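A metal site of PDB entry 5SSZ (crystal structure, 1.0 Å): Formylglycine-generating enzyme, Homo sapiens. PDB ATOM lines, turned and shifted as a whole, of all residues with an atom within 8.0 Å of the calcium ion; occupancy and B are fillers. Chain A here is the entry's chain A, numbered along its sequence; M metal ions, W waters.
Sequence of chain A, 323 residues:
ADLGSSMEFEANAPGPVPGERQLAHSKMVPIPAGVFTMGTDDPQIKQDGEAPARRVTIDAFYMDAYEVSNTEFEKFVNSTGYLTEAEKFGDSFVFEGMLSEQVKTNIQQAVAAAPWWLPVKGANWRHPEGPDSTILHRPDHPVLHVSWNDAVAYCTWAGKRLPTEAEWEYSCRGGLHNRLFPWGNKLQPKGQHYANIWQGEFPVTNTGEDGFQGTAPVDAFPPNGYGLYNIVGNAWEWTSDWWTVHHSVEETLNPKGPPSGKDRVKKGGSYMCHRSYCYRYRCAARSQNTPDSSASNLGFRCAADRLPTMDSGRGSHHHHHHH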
ATOM      1  N   HIS A 193      16.446 -20.097 -26.552  1.00  0.00           N
ATOM      2  CA  HIS A 193      15.100 -20.436 -26.089  1.00  0.00           C
ATOM      3  C   HIS A 193      14.131 -20.469 -27.264  1.00  0.00           C
ATOM      4  O   HIS A 193      14.106 -19.561 -28.100  1.00  0.00           O
ATOM      5  CB  HIS A 193      14.626 -19.448 -25.027  1.00  0.00           C
ATOM      6  CG  HIS A 193      15.280 -19.694 -23.706  1.00  0.00           C
ATOM      7  ND1 HIS A 193      14.863 -20.700 -22.860  1.00  0.00           N
ATOM      8  CD2 HIS A 193      16.364 -19.136 -23.133  1.00  0.00           C
ATOM      9  CE1 HIS A 193      15.657 -20.727 -21.818  1.00  0.00           C
ATOM     10  NE2 HIS A 193      16.575 -19.783 -21.948  1.00  0.00           N
ATOM     11  N   ALA A 195      10.662 -21.489 -26.657  1.00  0.00           N
ATOM     12  CA  ALA A 195       9.311 -21.395 -26.128  1.00  0.00           C
ATOM     13  C   ALA A 195       9.344 -20.700 -24.783  1.00  0.00           C
ATOM     14  O   ALA A 195      10.377 -20.679 -24.095  1.00  0.00           O
ATOM     15  CB  ALA A 195       8.668 -22.773 -25.982  1.00  0.00           C
ATOM     16  N   ASN A 196       8.198 -20.133 -24.407  1.00  0.00           N
ATOM     17  CA  ASN A 196       8.033 -19.429 -23.130  1.00  0.00           C
ATOM     18  C   ASN A 196       7.509 -20.403 -22.088  1.00  0.00           C
ATOM     19  O   ASN A 196       6.303 -20.702 -22.041  1.00  0.00           O
ATOM     20  CB  ASN A 196       7.074 -18.260 -23.322  1.00  0.00           C
ATOM     21  CG  ASN A 196       6.858 -17.489 -22.048  1.00  0.00           C
ATOM     22  OD1 ASN A 196       7.666 -17.593 -21.111  1.00  0.00           O
ATOM     23  ND2 ASN A 196       5.808 -16.685 -21.993  1.00  0.00           N
ATOM     24  N   ILE A 197       8.422 -20.896 -21.249  1.00  0.00           N
ATOM     25  CA  ILE A 197       8.087 -21.734 -20.100  1.00  0.00           C
ATOM     26  C   ILE A 197       8.763 -21.112 -18.869  1.00  0.00           C
ATOM     27  O   ILE A 197       9.173 -19.950 -18.898  1.00  0.00           O
ATOM     28  CB  ILE A 197       8.419 -23.225 -20.340  1.00  0.00           C
ATOM     29  CG1 ILE A 197       9.913 -23.471 -20.586  1.00  0.00           C
ATOM     30  CG2 ILE A 197       7.562 -23.758 -21.522  1.00  0.00           C
ATOM     31  CD1 ILE A 197      10.254 -24.948 -20.566  1.00  0.00           C
ATOM     32  N   TRP A 198       8.862 -21.852 -17.775  1.00  0.00           N
ATOM     33  CA  TRP A 198       9.451 -21.330 -16.539  1.00  0.00           C
ATOM     34  C   TRP A 198      10.936 -21.667 -16.509  1.00  0.00           C
ATOM     35  O   TRP A 198      11.330 -22.758 -16.910  1.00  0.00           O
ATOM     36  CB  TRP A 198       8.782 -22.029 -15.365  1.00  0.00           C
ATOM     37  CG  TRP A 198       9.092 -21.554 -13.983  1.00  0.00           C
ATOM     38  CD1 TRP A 198      10.196 -21.826 -13.227  1.00  0.00           C
ATOM     39  CD2 TRP A 198       8.235 -20.750 -13.167  1.00  0.00           C
ATOM     40  NE1 TRP A 198      10.073 -21.246 -11.983  1.00  0.00           N
ATOM     41  CE2 TRP A 198       8.890 -20.570 -11.927  1.00  0.00           C
ATOM     42  CE3 TRP A 198       6.980 -20.164 -13.357  1.00  0.00           C
ATOM     43  CZ2 TRP A 198       8.315 -19.841 -10.891  1.00  0.00           C
ATOM     44  CZ3 TRP A 198       6.427 -19.429 -12.326  1.00  0.00           C
ATOM     45  CH2 TRP A 198       7.077 -19.281 -11.102  1.00  0.00           C
ATOM     46  N   GLN A 199      11.768 -20.745 -16.003  1.00  0.00           N
ATOM     47  CA  GLN A 199      13.123 -21.075 -15.574  1.00  0.00           C
ATOM     48  C   GLN A 199      13.277 -20.660 -14.125  1.00  0.00           C
ATOM     49  O   GLN A 199      12.719 -19.645 -13.706  1.00  0.00           O
ATOM     50  CB  GLN A 199      14.210 -20.372 -16.396  1.00  0.00           C
ATOM     51  CG  GLN A 199      14.214 -20.756 -17.881  1.00  0.00           C
ATOM     52  CD  GLN A 199      13.218 -19.956 -18.691  1.00  0.00           C
ATOM     53  OE1 GLN A 199      13.066 -18.747 -18.489  1.00  0.00           O
ATOM     54  NE2 GLN A 199      12.539 -20.626 -19.613  1.00  0.00           N
ATOM     55  N   ASN A 206      10.767 -17.400 -10.753  1.00  0.00           N
ATOM     56  CA  ASN A 206      10.852 -17.459 -12.204  1.00  0.00           C
ATOM     57  C   ASN A 206      11.889 -16.433 -12.610  1.00  0.00           C
ATOM     58  O   ASN A 206      11.705 -15.226 -12.382  1.00  0.00           O
ATOM     59  CB  ASN A 206       9.495 -17.139 -12.825  1.00  0.00           C
ATOM     60  CG  ASN A 206       9.472 -17.379 -14.315  1.00  0.00           C
ATOM     61  OD1 ASN A 206      10.510 -17.562 -14.952  1.00  0.00           O
ATOM     62  ND2 ASN A 206       8.292 -17.398 -14.892  1.00  0.00           N
ATOM     63  N   THR A 207      13.010 -16.892 -13.167  1.00  0.00           N
ATOM     64  CA  THR A 207      14.077 -15.965 -13.493  1.00  0.00           C
ATOM     65  C   THR A 207      13.770 -15.110 -14.717  1.00  0.00           C
ATOM     66  O   THR A 207      14.449 -14.102 -14.933  1.00  0.00           O
ATOM     67  CB  THR A 207      15.390 -16.709 -13.736  1.00  0.00           C
ATOM     68  OG1 THR A 207      15.234 -17.493 -14.915  1.00  0.00           O
ATOM     69  CG2 THR A 207      15.757 -17.590 -12.556  1.00  0.00           C
ATOM     70  N   GLY A 208      12.806 -15.508 -15.555  1.00  0.00           N
ATOM     71  CA  GLY A 208      12.602 -14.765 -16.775  1.00  0.00           C
ATOM     72  C   GLY A 208      13.752 -14.857 -17.752  1.00  0.00           C
ATOM     73  O   GLY A 208      13.896 -13.981 -18.624  1.00  0.00           O
ATOM     74  N   GLU A 209      14.551 -15.918 -17.664  1.00  0.00           N
ATOM     75  CA  GLU A 209      15.693 -16.102 -18.563  1.00  0.00           C
ATOM     76  C   GLU A 209      15.276 -16.075 -20.031  1.00  0.00           C
ATOM     77  O   GLU A 209      16.005 -15.523 -20.863  1.00  0.00           O
ATOM     78  CB  GLU A 209      16.377 -17.429 -18.228  1.00  0.00           C
ATOM     79  CG  GLU A 209      17.543 -17.775 -19.111  1.00  0.00           C
ATOM     80  CD  GLU A 209      18.016 -19.194 -18.934  1.00  0.00           C
ATOM     81  OE1 GLU A 209      17.798 -19.768 -17.843  1.00  0.00           O
ATOM     82  OE2 GLU A 209      18.576 -19.747 -19.899  1.00  0.00           O
ATOM     83  N   ASP A 210      14.122 -16.676 -20.365  1.00  0.00           N
ATOM     84  CA  ASP A 210      13.660 -16.708 -21.750  1.00  0.00           C
ATOM     85  C   ASP A 210      13.074 -15.390 -22.224  1.00  0.00           C
ATOM     86  O   ASP A 210      12.627 -15.320 -23.378  1.00  0.00           O
ATOM     87  CB  ASP A 210      12.694 -17.877 -21.984  1.00  0.00           C
ATOM     88  CG  ASP A 210      11.407 -17.751 -21.208  1.00  0.00           C
ATOM     89  OD1 ASP A 210      11.036 -16.639 -20.785  1.00  0.00           O
ATOM     90  OD2 ASP A 210      10.743 -18.800 -21.015  1.00  0.00           O
ATOM     91  N   GLY A 211      13.053 -14.362 -21.381  1.00  0.00           N
ATOM     92  CA  GLY A 211      12.561 -13.055 -21.748  1.00  0.00           C
ATOM     93  C   GLY A 211      11.193 -12.696 -21.237  1.00  0.00           C
ATOM     94  O   GLY A 211      10.790 -11.528 -21.395  1.00  0.00           O
ATOM     95  N   PHE A 212      10.464 -13.638 -20.637  1.00  0.00           N
ATOM     96  CA  PHE A 212       9.081 -13.407 -20.223  1.00  0.00           C
ATOM     97  C   PHE A 212       8.779 -14.190 -18.956  1.00  0.00           C
ATOM     98  O   PHE A 212       8.929 -15.404 -18.934  1.00  0.00           O
ATOM     99  CB  PHE A 212       8.101 -13.806 -21.341  1.00  0.00           C
ATOM    100  CG  PHE A 212       8.391 -13.098 -22.620  1.00  0.00           C
ATOM    101  CD1 PHE A 212       7.876 -11.828 -22.858  1.00  0.00           C
ATOM    102  CD2 PHE A 212       9.250 -13.661 -23.546  1.00  0.00           C
ATOM    103  CE1 PHE A 212       8.217 -11.143 -24.021  1.00  0.00           C
ATOM    104  CE2 PHE A 212       9.579 -12.991 -24.699  1.00  0.00           C
ATOM    105  CZ  PHE A 212       9.072 -11.731 -24.932  1.00  0.00           C
ATOM    106  N   GLN A 213       8.339 -13.448 -17.935  1.00  0.00           N
ATOM    107  CA  GLN A 213       7.848 -14.024 -16.679  1.00  0.00           C
ATOM    108  C   GLN A 213       6.456 -14.606 -16.862  1.00  0.00           C
ATOM    109  O   GLN A 213       6.222 -15.786 -16.574  1.00  0.00           O
ATOM    110  CB  GLN A 213       7.798 -12.920 -15.624  1.00  0.00           C
ATOM    111  CG  GLN A 213       9.148 -12.492 -15.102  1.00  0.00           C
ATOM    112  CD  GLN A 213       9.618 -13.387 -13.989  1.00  0.00           C
ATOM    113  OE1 GLN A 213       8.837 -14.156 -13.433  1.00  0.00           O
ATOM    114  NE2 GLN A 213      10.900 -13.312 -13.660  1.00  0.00           N
ATOM    115  N   GLY A 214       5.506 -13.769 -17.287  1.00  0.00           N
ATOM    116  CA  GLY A 214       4.185 -14.169 -17.676  1.00  0.00           C
ATOM    117  C   GLY A 214       4.148 -14.492 -19.150  1.00  0.00           C
ATOM    118  O   GLY A 214       5.101 -15.050 -19.710  1.00  0.00           O
ATOM    119  N   THR A 215       3.050 -14.149 -19.809  1.00  0.00           N
ATOM    120  CA  THR A 215       2.932 -14.391 -21.234  1.00  0.00           C
ATOM    121  C   THR A 215       3.903 -13.521 -22.034  1.00  0.00           C
ATOM    122  O   THR A 215       4.428 -12.499 -21.575  1.00  0.00           O
ATOM    123  CB  THR A 215       1.511 -14.105 -21.716  1.00  0.00           C
ATOM    124  OG1 THR A 215       1.131 -12.760 -21.363  1.00  0.00           O
ATOM    125  CG2 THR A 215       0.504 -15.074 -21.111  1.00  0.00           C
ATOM    126  N   ALA A 216       4.119 -13.957 -23.265  1.00  0.00           N
ATOM    127  CA  ALA A 216       4.823 -13.245 -24.309  1.00  0.00           C
ATOM    128  C   ALA A 216       3.844 -12.875 -25.410  1.00  0.00           C
ATOM    129  O   ALA A 216       2.779 -13.488 -25.542  1.00  0.00           O
ATOM    130  CB  ALA A 216       5.894 -14.163 -24.915  1.00  0.00           C
ATOM    131  N   PHE A 221       9.120 -15.916 -30.242  1.00  0.00           N
ATOM    132  CA  PHE A 221       9.848 -17.177 -30.369  1.00  0.00           C
ATOM    133  C   PHE A 221       9.797 -17.698 -31.805  1.00  0.00           C
ATOM    134  O   PHE A 221       9.015 -17.212 -32.634  1.00  0.00           O
ATOM    135  CB  PHE A 221       9.417 -18.200 -29.302  1.00  0.00           C
ATOM    136  CG  PHE A 221       9.764 -17.745 -27.922  1.00  0.00           C
ATOM    137  CD1 PHE A 221      11.055 -17.882 -27.430  1.00  0.00           C
ATOM    138  CD2 PHE A 221       8.820 -17.120 -27.134  1.00  0.00           C
ATOM    139  CE1 PHE A 221      11.390 -17.416 -26.172  1.00  0.00           C
ATOM    140  CE2 PHE A 221       9.146 -16.649 -25.890  1.00  0.00           C
ATOM    141  CZ  PHE A 221      10.425 -16.798 -25.403  1.00  0.00           C
ATOM    142  N   ASN A 234       3.715 -20.595 -23.437  1.00  0.00           N
ATOM    143  CA  ASN A 234       2.964 -19.344 -23.489  1.00  0.00           C
ATOM    144  C   ASN A 234       1.597 -19.568 -22.826  1.00  0.00           C
ATOM    145  O   ASN A 234       1.537 -19.607 -21.585  1.00  0.00           O
ATOM    146  CB  ASN A 234       2.958 -18.683 -24.879  1.00  0.00           C
ATOM    147  CG  ASN A 234       2.992 -17.172 -24.784  1.00  0.00           C
ATOM    148  OD1 ASN A 234       3.579 -16.627 -23.842  1.00  0.00           O
ATOM    149  ND2 ASN A 234       2.389 -16.499 -25.757  1.00  0.00           N
ATOM    150  N   SER A 270       2.347 -24.074 -20.852  1.00  0.00           N
ATOM    151  CA  SER A 270       2.255 -22.626 -20.667  1.00  0.00           C
ATOM    152  C   SER A 270       3.563 -22.071 -20.125  1.00  0.00           C
ATOM    153  O   SER A 270       4.515 -22.804 -19.821  1.00  0.00           O
ATOM    154  CB  SER A 270       1.130 -22.243 -19.690  1.00  0.00           C
ATOM    155  OG  SER A 270       1.510 -22.413 -18.332  1.00  0.00           O
ATOM    156  N   TYR A 271       3.550 -20.753 -19.913  1.00  0.00           N
ATOM    157  CA  TYR A 271       4.666 -20.042 -19.293  1.00  0.00           C
ATOM    158  C   TYR A 271       5.003 -20.533 -17.892  1.00  0.00           C
ATOM    159  O   TYR A 271       6.094 -20.210 -17.389  1.00  0.00           O
ATOM    160  CB  TYR A 271       4.370 -18.539 -19.296  1.00  0.00           C
ATOM    161  CG  TYR A 271       3.311 -18.062 -18.320  1.00  0.00           C
ATOM    162  CD1 TYR A 271       3.619 -17.863 -16.983  1.00  0.00           C
ATOM    163  CD2 TYR A 271       2.045 -17.749 -18.767  1.00  0.00           C
ATOM    164  CE1 TYR A 271       2.676 -17.389 -16.092  1.00  0.00           C
ATOM    165  CE2 TYR A 271       1.085 -17.253 -17.866  1.00  0.00           C
ATOM    166  CZ  TYR A 271       1.429 -17.087 -16.533  1.00  0.00           C
ATOM    167  OH  TYR A 271       0.510 -16.584 -15.626  1.00  0.00           O
ATOM    168  N   MET A 272       4.109 -21.292 -17.255  1.00  0.00           N
ATOM    169  CA  MET A 272       4.367 -21.854 -15.937  1.00  0.00           C
ATOM    170  C   MET A 272       5.109 -23.182 -15.954  1.00  0.00           C
ATOM    171  O   MET A 272       5.584 -23.614 -14.899  1.00  0.00           O
ATOM    172  CB  MET A 272       3.058 -22.062 -15.169  1.00  0.00           C
ATOM    173  CG  MET A 272       2.356 -20.772 -14.850  1.00  0.00           C
ATOM    174  SD  MET A 272       0.711 -21.077 -14.172  1.00  0.00           S
ATOM    175  CE  MET A 272       1.110 -21.965 -12.664  1.00  0.00           C
ATOM    176  N   CYS A 273       5.188 -23.873 -17.083  1.00  0.00           N
ATOM    177  CA  CYS A 273       5.665 -25.254 -17.057  1.00  0.00           C
ATOM    178  C   CYS A 273       7.148 -25.326 -16.730  1.00  0.00           C
ATOM    179  O   CYS A 273       7.951 -24.501 -17.169  1.00  0.00           O
ATOM    180  CB  CYS A 273       5.463 -25.936 -18.413  1.00  0.00           C
ATOM    181  SG  CYS A 273       3.818 -26.381 -18.959  1.00  0.00           S
HETATM  182 CA    CA M   1       9.250 -17.677 -19.427  1.00  0.00          CA
HETATM  183  O   HOH W   1       7.549 -17.881 -17.745  1.00  0.00           O
HETATM  184  O   HOH W   2      10.824 -17.538 -17.655  1.00  0.00           O
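The calcium ion is bound by the side-chain amide oxygen (OD1) of Asn 196 (2.3 Å), the backbone carbonyl oxygen (O) of Ile 197 (2.3 Å), the backbone carbonyl oxygen (O) of Phe 212 (2.3 Å), water W2 (2.4 Å), water W1 (2.4 Å), the side-chain carboxylate (OD2) of Asp 210 (2.5 Å) and the side-chain carboxylate (OD1) of Asp 210 (2.5 Å).
Of the 23 residues printed, 4 come within 4 Å of the calcium ion.
Water W1 lies within hydrogen-bond range of the backbone carbonyl oxygen (O) of Gln 213, the backbone carbonyl oxygen (O) of Tyr 271 and the side-chain amide nitrogen (ND2) of Asn 206.
Water W2 bridges OE1 of Gln 199 (2.7 Å) and OD1 of Asn 206 (2.7 Å).
The side-chain amide nitrogen of Asn 196 lies within hydrogen-bond range of the backbone carbonyl oxygen of Gly 214 (2.9 Å).
The side-chain amide nitrogen (ND2) of Asn 196 lies close to the backbone NH (N) of Ala 216 (3.5 Å).
The backbone carbonyl oxygen (O) of Asn 196 lies close to the backbone NH (N) of Tyr 271, at 3.5 Å.
The side-chain amide oxygen of Gln 199 lies within hydrogen-bond range of the backbone NH of Asp 210, at 3.0 Å.
The side-chain amide nitrogen (ND2) of Asn 196 lies within hydrogen-bond range of the side-chain amide oxygen (OD1) of Asn 234 (2.9 Å).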
